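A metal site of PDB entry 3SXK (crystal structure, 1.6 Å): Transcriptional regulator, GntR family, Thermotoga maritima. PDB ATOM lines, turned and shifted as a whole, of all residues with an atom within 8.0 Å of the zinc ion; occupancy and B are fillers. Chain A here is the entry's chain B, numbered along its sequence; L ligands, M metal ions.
A ring nitrogen (NE2) of His 63 sits close to the side-chain carboxylate (OD1) of Asp 59 (3.3 Å). ND1 of His 63 lies within hydrogen-bond range of NH2 of Arg 15 (3.2 Å). A ring nitrogen (ND1) of His 63 lies within hydrogen-bond range of the side-chain carboxylate (OE1) of Glu 19. OD1 of Asp 59 lies close to NE2 of His 103 (3.2 Å). ND1 of His 103 sits close to O of Ser 99 (3.4 Å). OE1 of Glu 102 sits at hydrogen-bond distance from ND1 of His 125 (2.7 Å). OD2 of Asp 59 lies within salt-bridge range of NH1 of Arg 90 (2.8 Å).
The zinc ion is bound by NE2 of His 63, NE2 of His 103, NE2 of His 125 and O3 of the ligand. Slightly farther from the zinc ion lies the side-chain carboxylate (OD1) of Asp 59 (2.8 Å).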
ATOM      1  N   ARG A  15       5.559  28.268  -0.638  1.00  0.00           N
ATOM      2  CA  ARG A  15       5.617  27.474   0.592  1.00  0.00           C
ATOM      3  C   ARG A  15       4.354  26.678   0.857  1.00  0.00           C
ATOM      4  O   ARG A  15       4.423  25.502   1.224  1.00  0.00           O
ATOM      5  CB  ARG A  15       5.937  28.348   1.802  1.00  0.00           C
ATOM      6  CG  ARG A  15       7.278  29.034   1.734  1.00  0.00           C
ATOM      7  CD  ARG A  15       7.553  29.824   3.007  1.00  0.00           C
ATOM      8  NE  ARG A  15       7.705  28.977   4.158  1.00  0.00           N
ATOM      9  CZ  ARG A  15       7.784  29.437   5.411  1.00  0.00           C
ATOM     10  NH1 ARG A  15       7.833  30.766   5.605  1.00  0.00           N
ATOM     11  NH2 ARG A  15       7.854  28.587   6.409  1.00  0.00           N
ATOM     12  N   GLU A  19       4.880  22.781   1.185  1.00  0.00           N
ATOM     13  CA  GLU A  19       4.808  22.277   2.556  1.00  0.00           C
ATOM     14  C   GLU A  19       3.484  21.570   2.827  1.00  0.00           C
ATOM     15  O   GLU A  19       3.463  20.544   3.494  1.00  0.00           O
ATOM     16  CB  GLU A  19       4.986  23.397   3.588  1.00  0.00           C
ATOM     17  CG  GLU A  19       6.351  24.099   3.544  1.00  0.00           C
ATOM     18  CD  GLU A  19       6.503  25.152   4.623  1.00  0.00           C
ATOM     19  OE1 GLU A  19       5.801  25.014   5.661  1.00  0.00           O
ATOM     20  OE2 GLU A  19       7.344  26.081   4.480  1.00  0.00           O
ATOM     21  N   PHE A  55      12.556  30.592  18.554  1.00  0.00           N
ATOM     22  CA  PHE A  55      12.007  30.666  17.198  1.00  0.00           C
ATOM     23  C   PHE A  55      12.899  30.235  16.032  1.00  0.00           C
ATOM     24  O   PHE A  55      12.521  29.339  15.308  1.00  0.00           O
ATOM     25  CB  PHE A  55      11.413  32.055  16.902  1.00  0.00           C
ATOM     26  CG  PHE A  55      10.789  32.163  15.535  1.00  0.00           C
ATOM     27  CD1 PHE A  55       9.435  31.867  15.317  1.00  0.00           C
ATOM     28  CD2 PHE A  55      11.564  32.522  14.446  1.00  0.00           C
ATOM     29  CE1 PHE A  55       8.890  31.958  14.079  1.00  0.00           C
ATOM     30  CE2 PHE A  55      11.002  32.596  13.170  1.00  0.00           C
ATOM     31  CZ  PHE A  55       9.660  32.318  13.003  1.00  0.00           C
ATOM     32  N   SER A  58      13.751  26.452  15.964  1.00  0.00           N
ATOM     33  CA  SER A  58      12.557  25.580  15.853  1.00  0.00           C
ATOM     34  C   SER A  58      11.763  25.798  14.558  1.00  0.00           C
ATOM     35  O   SER A  58      11.209  24.860  14.015  1.00  0.00           O
ATOM     36  CB  SER A  58      11.597  25.659  17.050  1.00  0.00           C
ATOM     37  OG  SER A  58      10.988  26.938  17.196  1.00  0.00           O
ATOM     38  N   ASP A  59      11.674  27.040  14.108  1.00  0.00           N
ATOM     39  CA  ASP A  59      10.921  27.382  12.917  1.00  0.00           C
ATOM     40  C   ASP A  59      11.467  26.722  11.666  1.00  0.00           C
ATOM     41  O   ASP A  59      10.722  25.984  10.987  1.00  0.00           O
ATOM     42  CB  ASP A  59      10.883  28.898  12.689  1.00  0.00           C
ATOM     43  CG  ASP A  59      10.159  29.267  11.392  1.00  0.00           C
ATOM     44  OD1 ASP A  59       8.983  28.943  11.295  1.00  0.00           O
ATOM     45  OD2 ASP A  59      10.767  29.783  10.429  1.00  0.00           O
ATOM     46  N   GLU A  60      12.758  26.903  11.390  1.00  0.00           N
ATOM     47  CA  GLU A  60      13.363  26.278  10.225  1.00  0.00           C
ATOM     48  C   GLU A  60      13.227  24.753  10.299  1.00  0.00           C
ATOM     49  O   GLU A  60      12.919  24.086   9.305  1.00  0.00           O
ATOM     50  CB  GLU A  60      14.844  26.679  10.105  1.00  0.00           C
ATOM     51  CG  GLU A  60      15.571  25.925   9.018  1.00  0.00           C
ATOM     52  CD  GLU A  60      16.958  26.415   8.680  1.00  0.00           C
ATOM     53  OE1 GLU A  60      17.487  27.312   9.354  1.00  0.00           O
ATOM     54  OE2 GLU A  60      17.534  25.887   7.698  1.00  0.00           O
ATOM     55  N   LEU A  62      10.967  22.872  11.832  1.00  0.00           N
ATOM     56  CA  LEU A  62       9.627  22.376  11.695  1.00  0.00           C
ATOM     57  C   LEU A  62       9.200  22.392  10.196  1.00  0.00           C
ATOM     58  O   LEU A  62       8.693  21.400   9.669  1.00  0.00           O
ATOM     59  CB  LEU A  62       8.658  23.223  12.530  1.00  0.00           C
ATOM     60  CG  LEU A  62       7.195  22.795  12.474  1.00  0.00           C
ATOM     61  CD1 LEU A  62       6.970  21.346  12.937  1.00  0.00           C
ATOM     62  CD2 LEU A  62       6.254  23.747  13.229  1.00  0.00           C
ATOM     63  N   HIS A  63       9.400  23.524   9.532  1.00  0.00           N
ATOM     64  CA  HIS A  63       8.999  23.638   8.131  1.00  0.00           C
ATOM     65  C   HIS A  63       9.839  22.707   7.244  1.00  0.00           C
ATOM     66  O   HIS A  63       9.305  22.056   6.344  1.00  0.00           O
ATOM     67  CB  HIS A  63       9.083  25.096   7.682  1.00  0.00           C
ATOM     68  CG  HIS A  63       8.009  25.967   8.291  1.00  0.00           C
ATOM     69  ND1 HIS A  63       6.710  25.967   7.840  1.00  0.00           N
ATOM     70  CD2 HIS A  63       8.044  26.856   9.320  1.00  0.00           C
ATOM     71  CE1 HIS A  63       5.986  26.809   8.559  1.00  0.00           C
ATOM     72  NE2 HIS A  63       6.781  27.367   9.457  1.00  0.00           N
ATOM     73  N   PHE A  66       8.700  18.922   7.286  1.00  0.00           N
ATOM     74  CA  PHE A  66       7.563  18.517   6.475  1.00  0.00           C
ATOM     75  C   PHE A  66       8.079  18.097   5.071  1.00  0.00           C
ATOM     76  O   PHE A  66       7.650  17.098   4.533  1.00  0.00           O
ATOM     77  CB  PHE A  66       6.566  19.660   6.326  1.00  0.00           C
ATOM     78  CG  PHE A  66       5.950  20.151   7.633  1.00  0.00           C
ATOM     79  CD1 PHE A  66       5.817  19.321   8.734  1.00  0.00           C
ATOM     80  CD2 PHE A  66       5.577  21.472   7.742  1.00  0.00           C
ATOM     81  CE1 PHE A  66       5.275  19.801   9.928  1.00  0.00           C
ATOM     82  CE2 PHE A  66       5.026  21.975   8.930  1.00  0.00           C
ATOM     83  CZ  PHE A  66       4.878  21.130  10.018  1.00  0.00           C
ATOM     84  N   ARG A  90      10.897  35.762   6.078  1.00  0.00           N
ATOM     85  CA  ARG A  90      10.561  35.580   7.490  1.00  0.00           C
ATOM     86  C   ARG A  90      11.184  36.663   8.341  1.00  0.00           C
ATOM     87  O   ARG A  90      10.613  37.043   9.358  1.00  0.00           O
ATOM     88  CB  ARG A  90      10.863  34.188   8.043  1.00  0.00           C
ATOM     89  CG  ARG A  90      12.257  33.837   8.210  1.00  0.00           C
ATOM     90  CD  ARG A  90      12.371  32.318   8.673  1.00  0.00           C
ATOM     91  NE  ARG A  90      13.776  32.032   8.903  1.00  0.00           N
ATOM     92  CZ  ARG A  90      14.268  31.171   9.779  1.00  0.00           C
ATOM     93  NH1 ARG A  90      13.495  30.398  10.538  1.00  0.00           N
ATOM     94  NH2 ARG A  90      15.576  31.014   9.849  1.00  0.00           N
ATOM     95  N   ARG A  95       7.544  38.049  14.334  1.00  0.00           N
ATOM     96  CA  ARG A  95       6.317  37.531  14.939  1.00  0.00           C
ATOM     97  C   ARG A  95       6.563  36.356  15.864  1.00  0.00           C
ATOM     98  O   ARG A  95       5.772  35.412  15.937  1.00  0.00           O
ATOM     99  CB  ARG A  95       5.414  37.177  13.763  1.00  0.00           C
ATOM    100  CG  ARG A  95       3.979  36.978  14.077  1.00  0.00           C
ATOM    101  CD  ARG A  95       3.209  36.901  12.772  1.00  0.00           C
ATOM    102  NE  ARG A  95       1.793  36.616  12.960  1.00  0.00           N
ATOM    103  CZ  ARG A  95       1.269  35.383  12.976  1.00  0.00           C
ATOM    104  NH1 ARG A  95       2.038  34.308  12.841  1.00  0.00           N
ATOM    105  NH2 ARG A  95      -0.060  35.246  13.123  1.00  0.00           N
ATOM    106  N   SER A  99       3.896  33.348  16.040  1.00  0.00           N
ATOM    107  CA  SER A  99       4.238  32.217  15.185  1.00  0.00           C
ATOM    108  C   SER A  99       4.568  30.968  15.998  1.00  0.00           C
ATOM    109  O   SER A  99       4.246  29.855  15.592  1.00  0.00           O
ATOM    110  CB  SER A  99       5.374  32.583  14.202  1.00  0.00           C
ATOM    111  OG  SER A  99       4.833  33.397  13.183  1.00  0.00           O
ATOM    112  N   ASN A 100       5.199  31.172  17.148  1.00  0.00           N
ATOM    113  CA  ASN A 100       5.520  30.079  18.025  1.00  0.00           C
ATOM    114  C   ASN A 100       4.229  29.373  18.465  1.00  0.00           C
ATOM    115  O   ASN A 100       4.177  28.145  18.434  1.00  0.00           O
ATOM    116  CB  ASN A 100       6.321  30.515  19.228  1.00  0.00           C
ATOM    117  CG  ASN A 100       6.830  29.358  20.029  1.00  0.00           C
ATOM    118  OD1 ASN A 100       7.408  28.411  19.477  1.00  0.00           O
ATOM    119  ND2 ASN A 100       6.605  29.401  21.344  1.00  0.00           N
ATOM    120  N   GLU A 102       1.342  29.329  16.996  1.00  0.00           N
ATOM    121  CA  GLU A 102       0.803  28.624  15.825  1.00  0.00           C
ATOM    122  C   GLU A 102       1.540  27.324  15.543  1.00  0.00           C
ATOM    123  O   GLU A 102       0.903  26.322  15.246  1.00  0.00           O
ATOM    124  CB  GLU A 102       0.826  29.541  14.615  1.00  0.00           C
ATOM    125  CG  GLU A 102      -0.253  30.633  14.728  1.00  0.00           C
ATOM    126  CD  GLU A 102      -0.189  31.736  13.673  1.00  0.00           C
ATOM    127  OE1 GLU A 102       0.755  31.752  12.820  1.00  0.00           O
ATOM    128  OE2 GLU A 102      -1.064  32.633  13.717  1.00  0.00           O
ATOM    129  N   HIS A 103       2.841  27.320  15.639  1.00  0.00           N
ATOM    130  CA  HIS A 103       3.629  26.115  15.536  1.00  0.00           C
ATOM    131  C   HIS A 103       3.222  25.072  16.560  1.00  0.00           C
ATOM    132  O   HIS A 103       3.056  23.946  16.262  1.00  0.00           O
ATOM    133  CB  HIS A 103       5.106  26.409  15.708  1.00  0.00           C
ATOM    134  CG  HIS A 103       5.690  27.208  14.607  1.00  0.00           C
ATOM    135  ND1 HIS A 103       6.876  27.872  14.727  1.00  0.00           N
ATOM    136  CD2 HIS A 103       5.271  27.421  13.347  1.00  0.00           C
ATOM    137  CE1 HIS A 103       7.145  28.482  13.585  1.00  0.00           C
ATOM    138  NE2 HIS A 103       6.182  28.231  12.747  1.00  0.00           N
ATOM    139  N   LEU A 106      -0.027  23.568  15.718  1.00  0.00           N
ATOM    140  CA  LEU A 106       0.144  22.736  14.521  1.00  0.00           C
ATOM    141  C   LEU A 106       0.686  21.391  14.954  1.00  0.00           C
ATOM    142  O   LEU A 106       0.173  20.356  14.597  1.00  0.00           O
ATOM    143  CB  LEU A 106       1.078  23.451  13.511  1.00  0.00           C
ATOM    144  CG  LEU A 106       1.488  22.640  12.295  1.00  0.00           C
ATOM    145  CD1 LEU A 106       0.312  22.002  11.581  1.00  0.00           C
ATOM    146  CD2 LEU A 106       2.304  23.508  11.332  1.00  0.00           C
ATOM    147  N   LEU A 122      -1.611  24.614   9.126  1.00  0.00           N
ATOM    148  CA  LEU A 122      -0.415  25.036   8.382  1.00  0.00           C
ATOM    149  C   LEU A 122      -0.765  26.126   7.377  1.00  0.00           C
ATOM    150  O   LEU A 122      -0.072  27.113   7.220  1.00  0.00           O
ATOM    151  CB  LEU A 122       0.228  23.843   7.641  1.00  0.00           C
ATOM    152  CG  LEU A 122       1.444  24.235   6.816  1.00  0.00           C
ATOM    153  CD1 LEU A 122       2.487  25.024   7.631  1.00  0.00           C
ATOM    154  CD2 LEU A 122       2.058  22.936   6.262  1.00  0.00           C
ATOM    155  N   HIS A 125      -1.557  29.327   9.313  1.00  0.00           N
ATOM    156  CA  HIS A 125      -0.278  29.858   9.808  1.00  0.00           C
ATOM    157  C   HIS A 125       0.472  30.652   8.727  1.00  0.00           C
ATOM    158  O   HIS A 125       0.804  31.804   8.926  1.00  0.00           O
ATOM    159  CB  HIS A 125       0.576  28.716  10.389  1.00  0.00           C
ATOM    160  CG  HIS A 125       1.999  29.070  10.618  1.00  0.00           C
ATOM    161  ND1 HIS A 125       2.391  30.114  11.423  1.00  0.00           N
ATOM    162  CD2 HIS A 125       3.136  28.496  10.158  1.00  0.00           C
ATOM    163  CE1 HIS A 125       3.718  30.158  11.451  1.00  0.00           C
ATOM    164  NE2 HIS A 125       4.190  29.221  10.657  1.00  0.00           N
ATOM    165  N   LEU A 126       0.698  30.030   7.557  1.00  0.00           N
ATOM    166  CA  LEU A 126       1.392  30.723   6.488  1.00  0.00           C
ATOM    167  C   LEU A 126       0.620  31.952   5.985  1.00  0.00           C
ATOM    168  O   LEU A 126       1.207  32.981   5.731  1.00  0.00           O
ATOM    169  CB  LEU A 126       1.676  29.740   5.336  1.00  0.00           C
ATOM    170  CG  LEU A 126       2.760  28.702   5.733  1.00  0.00           C
ATOM    171  CD1 LEU A 126       2.849  27.556   4.721  1.00  0.00           C
ATOM    172  CD2 LEU A 126       4.162  29.372   5.941  1.00  0.00           C
ATOM    173  N   VAL A 129       1.026  34.686   8.558  1.00  0.00           N
ATOM    174  CA  VAL A 129       2.362  35.276   8.455  1.00  0.00           C
ATOM    175  C   VAL A 129       2.391  36.242   7.269  1.00  0.00           C
ATOM    176  O   VAL A 129       2.884  37.367   7.362  1.00  0.00           O
ATOM    177  CB  VAL A 129       3.445  34.164   8.307  1.00  0.00           C
ATOM    178  CG1 VAL A 129       4.747  34.740   7.833  1.00  0.00           C
ATOM    179  CG2 VAL A 129       3.609  33.427   9.626  1.00  0.00           C
HETATM  180  S1  LIG L   1       7.583  31.369   9.260  1.00  0.00           S
HETATM  181  O1  LIG L   1       8.132  32.699   9.583  1.00  0.00           O
HETATM  182  O2  LIG L   1       8.655  30.387   8.828  1.00  0.00           O
HETATM  183  O3  LIG L   1       6.892  30.832  10.498  1.00  0.00           O
HETATM  184  O4  LIG L   1       6.694  31.652   8.167  1.00  0.00           O
HETATM  185 ZN    ZN M   1       6.258  28.831  10.776  1.00  0.00          ZN
